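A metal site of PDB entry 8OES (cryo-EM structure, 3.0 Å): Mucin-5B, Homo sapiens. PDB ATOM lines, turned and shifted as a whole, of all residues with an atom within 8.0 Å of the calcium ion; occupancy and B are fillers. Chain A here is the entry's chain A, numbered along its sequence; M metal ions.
N of Asn 176 lies within hydrogen-bond range of O of Asp 184 (3.0 Å).
OD1 of Asn 186 lies close to OD2 of Asp 64, 3.5 Å away.
ND2 of Asn 192 sits at hydrogen-bond distance from OD2 of Asp 184.
ND2 of Asn 192 sits close to ND2 of Asn 186 (2.9 Å).
The backbone NH (N) of Asp 64 lies close to the side-chain hydroxyl (OG1) of Thr 62.
Asp 64 touches the calcium ion (OD2 to CA, 3.2 Å).
Asn 192 touches the calcium ion.
Six residues have an atom within 4 Å of the calcium ion: Asp 64, Asp 184, Asn 186, Leu 188, Asn 192 and Glu 193.
The nearest printed residue that does not touch the calcium ion is Pro 189 (4.5 Å).
The calcium ion is bound by OE1 of Glu 193, at 2.2 Å.
The calcium ion is bound by OD1 of Asn 186 (2.3 Å).
O of Leu 188 is bound to the calcium ion (2.3 Å).
The calcium ion is bound by ND2 of Asn 186 (2.8 Å).
The calcium ion is bound by OD1 of Asp 184, 2.8 Å away.
Slightly farther from the calcium ion lies OD2 of Asp 184 (3.0 Å).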
ATOM      1  N   THR A  62      13.219  -7.265 -21.306  1.00  0.00           N
ATOM      2  CA  THR A  62      14.525  -7.228 -21.926  1.00  0.00           C
ATOM      3  C   THR A  62      14.630  -8.293 -23.008  1.00  0.00           C
ATOM      4  O   THR A  62      13.713  -9.081 -23.238  1.00  0.00           O
ATOM      5  CB  THR A  62      15.623  -7.429 -20.883  1.00  0.00           C
ATOM      6  OG1 THR A  62      15.891  -8.834 -20.735  1.00  0.00           O
ATOM      7  CG2 THR A  62      15.220  -6.839 -19.546  1.00  0.00           C
ATOM      8  N   PHE A  63      15.781  -8.329 -23.685  1.00  0.00           N
ATOM      9  CA  PHE A  63      15.957  -9.251 -24.802  1.00  0.00           C
ATOM     10  C   PHE A  63      15.830 -10.697 -24.350  1.00  0.00           C
ATOM     11  O   PHE A  63      15.207 -11.517 -25.043  1.00  0.00           O
ATOM     12  CB  PHE A  63      17.324  -9.045 -25.449  1.00  0.00           C
ATOM     13  CG  PHE A  63      17.490  -7.706 -26.087  1.00  0.00           C
ATOM     14  CD1 PHE A  63      16.486  -7.161 -26.856  1.00  0.00           C
ATOM     15  CD2 PHE A  63      18.672  -7.016 -25.940  1.00  0.00           C
ATOM     16  CE1 PHE A  63      16.654  -5.936 -27.451  1.00  0.00           C
ATOM     17  CE2 PHE A  63      18.852  -5.795 -26.529  1.00  0.00           C
ATOM     18  CZ  PHE A  63      17.832  -5.251 -27.284  1.00  0.00           C
ATOM     19  N   ASP A  64      16.406 -11.037 -23.209  1.00  0.00           N
ATOM     20  CA  ASP A  64      16.617 -12.429 -22.825  1.00  0.00           C
ATOM     21  C   ASP A  64      15.432 -13.020 -22.073  1.00  0.00           C
ATOM     22  O   ASP A  64      15.477 -14.195 -21.707  1.00  0.00           O
ATOM     23  CB  ASP A  64      17.893 -12.544 -22.001  1.00  0.00           C
ATOM     24  CG  ASP A  64      18.856 -11.421 -22.276  1.00  0.00           C
ATOM     25  OD1 ASP A  64      19.005 -11.043 -23.461  1.00  0.00           O
ATOM     26  OD2 ASP A  64      19.473 -10.911 -21.318  1.00  0.00           O
ATOM     27  N   ASP A  66      13.514 -11.263 -19.370  1.00  0.00           N
ATOM     28  CA  ASP A  66      13.144 -10.667 -18.105  1.00  0.00           C
ATOM     29  C   ASP A  66      11.959  -9.721 -18.264  1.00  0.00           C
ATOM     30  O   ASP A  66      11.709  -9.183 -19.344  1.00  0.00           O
ATOM     31  CB  ASP A  66      14.320  -9.919 -17.494  1.00  0.00           C
ATOM     32  CG  ASP A  66      15.419 -10.849 -17.091  1.00  0.00           C
ATOM     33  OD1 ASP A  66      15.325 -12.045 -17.425  1.00  0.00           O
ATOM     34  OD2 ASP A  66      16.381 -10.397 -16.458  1.00  0.00           O
ATOM     35  N   ASN A 176      25.643  -8.753 -26.838  1.00  0.00           N
ATOM     36  CA  ASN A 176      26.675  -8.514 -25.830  1.00  0.00           C
ATOM     37  C   ASN A 176      27.298  -7.120 -25.938  1.00  0.00           C
ATOM     38  O   ASN A 176      28.116  -6.752 -25.100  1.00  0.00           O
ATOM     39  CB  ASN A 176      27.769  -9.570 -25.916  1.00  0.00           C
ATOM     40  CG  ASN A 176      28.284  -9.986 -24.559  1.00  0.00           C
ATOM     41  OD1 ASN A 176      27.930  -9.395 -23.543  1.00  0.00           O
ATOM     42  ND2 ASN A 176      29.132 -11.006 -24.545  1.00  0.00           N
ATOM     43  N   CYS A 182      16.763  -2.477 -22.110  1.00  0.00           N
ATOM     44  CA  CYS A 182      16.555  -3.697 -22.881  1.00  0.00           C
ATOM     45  C   CYS A 182      17.579  -4.774 -22.563  1.00  0.00           C
ATOM     46  O   CYS A 182      17.433  -5.894 -23.061  1.00  0.00           O
ATOM     47  CB  CYS A 182      16.564  -3.394 -24.387  1.00  0.00           C
ATOM     48  SG  CYS A 182      15.148  -2.444 -24.986  1.00  0.00           S
ATOM     49  N   GLY A 183      18.599  -4.476 -21.785  1.00  0.00           N
ATOM     50  CA  GLY A 183      19.504  -5.514 -21.334  1.00  0.00           C
ATOM     51  C   GLY A 183      20.820  -5.548 -22.079  1.00  0.00           C
ATOM     52  O   GLY A 183      21.241  -4.527 -22.622  1.00  0.00           O
ATOM     53  N   ASP A 184      21.467  -6.711 -22.118  1.00  0.00           N
ATOM     54  CA  ASP A 184      22.751  -6.822 -22.796  1.00  0.00           C
ATOM     55  C   ASP A 184      22.734  -7.704 -24.026  1.00  0.00           C
ATOM     56  O   ASP A 184      23.739  -7.744 -24.735  1.00  0.00           O
ATOM     57  CB  ASP A 184      23.823  -7.370 -21.844  1.00  0.00           C
ATOM     58  CG  ASP A 184      23.359  -8.588 -21.092  1.00  0.00           C
ATOM     59  OD1 ASP A 184      22.432  -9.250 -21.591  1.00  0.00           O
ATOM     60  OD2 ASP A 184      23.939  -8.896 -20.028  1.00  0.00           O
ATOM     61  N   PHE A 185      21.647  -8.438 -24.298  1.00  0.00           N
ATOM     62  CA  PHE A 185      21.543  -9.274 -25.495  1.00  0.00           C
ATOM     63  C   PHE A 185      22.594 -10.378 -25.520  1.00  0.00           C
ATOM     64  O   PHE A 185      23.030 -10.818 -26.586  1.00  0.00           O
ATOM     65  CB  PHE A 185      21.614  -8.425 -26.763  1.00  0.00           C
ATOM     66  CG  PHE A 185      21.021  -9.070 -27.978  1.00  0.00           C
ATOM     67  CD1 PHE A 185      20.297 -10.239 -27.889  1.00  0.00           C
ATOM     68  CD2 PHE A 185      21.183  -8.491 -29.222  1.00  0.00           C
ATOM     69  CE1 PHE A 185      19.764 -10.824 -29.003  1.00  0.00           C
ATOM     70  CE2 PHE A 185      20.650  -9.075 -30.349  1.00  0.00           C
ATOM     71  CZ  PHE A 185      19.932 -10.242 -30.240  1.00  0.00           C
ATOM     72  N   ASN A 186      23.006 -10.843 -24.333  1.00  0.00           N
ATOM     73  CA  ASN A 186      23.910 -11.978 -24.235  1.00  0.00           C
ATOM     74  C   ASN A 186      23.169 -13.305 -24.177  1.00  0.00           C
ATOM     75  O   ASN A 186      23.809 -14.362 -24.195  1.00  0.00           O
ATOM     76  CB  ASN A 186      24.805 -11.845 -23.003  1.00  0.00           C
ATOM     77  CG  ASN A 186      24.016 -11.780 -21.717  1.00  0.00           C
ATOM     78  OD1 ASN A 186      22.794 -11.892 -21.713  1.00  0.00           O
ATOM     79  ND2 ASN A 186      24.717 -11.594 -20.604  1.00  0.00           N
ATOM     80  N   GLY A 187      21.843 -13.275 -24.091  1.00  0.00           N
ATOM     81  CA  GLY A 187      21.030 -14.467 -24.058  1.00  0.00           C
ATOM     82  C   GLY A 187      20.727 -15.022 -22.695  1.00  0.00           C
ATOM     83  O   GLY A 187      19.836 -15.880 -22.576  1.00  0.00           O
ATOM     84  N   LEU A 188      21.404 -14.549 -21.656  1.00  0.00           N
ATOM     85  CA  LEU A 188      21.191 -15.061 -20.308  1.00  0.00           C
ATOM     86  C   LEU A 188      20.300 -14.098 -19.545  1.00  0.00           C
ATOM     87  O   LEU A 188      20.749 -13.007 -19.156  1.00  0.00           O
ATOM     88  CB  LEU A 188      22.524 -15.239 -19.581  1.00  0.00           C
ATOM     89  CG  LEU A 188      23.436 -16.282 -20.236  1.00  0.00           C
ATOM     90  CD1 LEU A 188      24.835 -16.199 -19.672  1.00  0.00           C
ATOM     91  CD2 LEU A 188      22.868 -17.669 -20.023  1.00  0.00           C
ATOM     92  N   PRO A 189      19.047 -14.450 -19.293  1.00  0.00           N
ATOM     93  CA  PRO A 189      18.099 -13.488 -18.734  1.00  0.00           C
ATOM     94  C   PRO A 189      18.383 -13.111 -17.294  1.00  0.00           C
ATOM     95  O   PRO A 189      18.552 -11.934 -16.970  1.00  0.00           O
ATOM     96  CB  PRO A 189      16.750 -14.204 -18.842  1.00  0.00           C
ATOM     97  CG  PRO A 189      17.043 -15.621 -19.072  1.00  0.00           C
ATOM     98  CD  PRO A 189      18.431 -15.758 -19.584  1.00  0.00           C
ATOM     99  N   ALA A 190      18.461 -14.105 -16.421  1.00  0.00           N
ATOM    100  CA  ALA A 190      18.303 -13.889 -14.994  1.00  0.00           C
ATOM    101  C   ALA A 190      19.604 -13.567 -14.278  1.00  0.00           C
ATOM    102  O   ALA A 190      19.593 -13.476 -13.046  1.00  0.00           O
ATOM    103  CB  ALA A 190      17.657 -15.120 -14.351  1.00  0.00           C
ATOM    104  N   PHE A 191      20.727 -13.397 -14.984  1.00  0.00           N
ATOM    105  CA  PHE A 191      21.983 -13.446 -14.247  1.00  0.00           C
ATOM    106  C   PHE A 191      22.857 -12.225 -14.542  1.00  0.00           C
ATOM    107  O   PHE A 191      23.676 -11.844 -13.697  1.00  0.00           O
ATOM    108  CB  PHE A 191      22.700 -14.781 -14.589  1.00  0.00           C
ATOM    109  CG  PHE A 191      24.204 -14.758 -14.485  1.00  0.00           C
ATOM    110  CD1 PHE A 191      24.963 -15.379 -15.457  1.00  0.00           C
ATOM    111  CD2 PHE A 191      24.838 -14.313 -13.340  1.00  0.00           C
ATOM    112  CE1 PHE A 191      26.335 -15.415 -15.354  1.00  0.00           C
ATOM    113  CE2 PHE A 191      26.209 -14.325 -13.235  1.00  0.00           C
ATOM    114  CZ  PHE A 191      26.955 -14.890 -14.239  1.00  0.00           C
ATOM    115  N   ASN A 192      22.663 -11.544 -15.672  1.00  0.00           N
ATOM    116  CA  ASN A 192      23.667 -10.548 -15.998  1.00  0.00           C
ATOM    117  C   ASN A 192      23.149  -9.124 -16.187  1.00  0.00           C
ATOM    118  O   ASN A 192      23.944  -8.193 -16.377  1.00  0.00           O
ATOM    119  CB  ASN A 192      24.422 -10.976 -17.249  1.00  0.00           C
ATOM    120  CG  ASN A 192      25.760 -10.300 -17.362  1.00  0.00           C
ATOM    121  OD1 ASN A 192      26.381  -9.965 -16.359  1.00  0.00           O
ATOM    122  ND2 ASN A 192      26.211 -10.082 -18.587  1.00  0.00           N
ATOM    123  N   GLU A 193      21.837  -8.911 -16.097  1.00  0.00           N
ATOM    124  CA  GLU A 193      21.333  -7.543 -16.241  1.00  0.00           C
ATOM    125  C   GLU A 193      21.451  -6.754 -14.948  1.00  0.00           C
ATOM    126  O   GLU A 193      21.593  -5.531 -14.990  1.00  0.00           O
ATOM    127  CB  GLU A 193      19.866  -7.537 -16.670  1.00  0.00           C
ATOM    128  CG  GLU A 193      19.537  -8.204 -17.992  1.00  0.00           C
ATOM    129  CD  GLU A 193      20.692  -8.263 -18.954  1.00  0.00           C
ATOM    130  OE1 GLU A 193      21.022  -9.389 -19.394  1.00  0.00           O
ATOM    131  OE2 GLU A 193      21.251  -7.207 -19.308  1.00  0.00           O
ATOM    132  N   PHE A 194      21.404  -7.440 -13.798  1.00  0.00           N
ATOM    133  CA  PHE A 194      21.254  -6.811 -12.494  1.00  0.00           C
ATOM    134  C   PHE A 194      22.414  -7.142 -11.574  1.00  0.00           C
ATOM    135  O   PHE A 194      22.206  -7.535 -10.431  1.00  0.00           O
ATOM    136  CB  PHE A 194      19.936  -7.217 -11.840  1.00  0.00           C
ATOM    137  CG  PHE A 194      18.853  -7.507 -12.822  1.00  0.00           C
ATOM    138  CD1 PHE A 194      18.699  -8.783 -13.329  1.00  0.00           C
ATOM    139  CD2 PHE A 194      18.001  -6.507 -13.241  1.00  0.00           C
ATOM    140  CE1 PHE A 194      17.704  -9.052 -14.227  1.00  0.00           C
ATOM    141  CE2 PHE A 194      17.007  -6.776 -14.139  1.00  0.00           C
ATOM    142  CZ  PHE A 194      16.858  -8.048 -14.639  1.00  0.00           C
HETATM  143 CA    CA M   1      22.143 -11.234 -19.608  1.00  0.00          CA
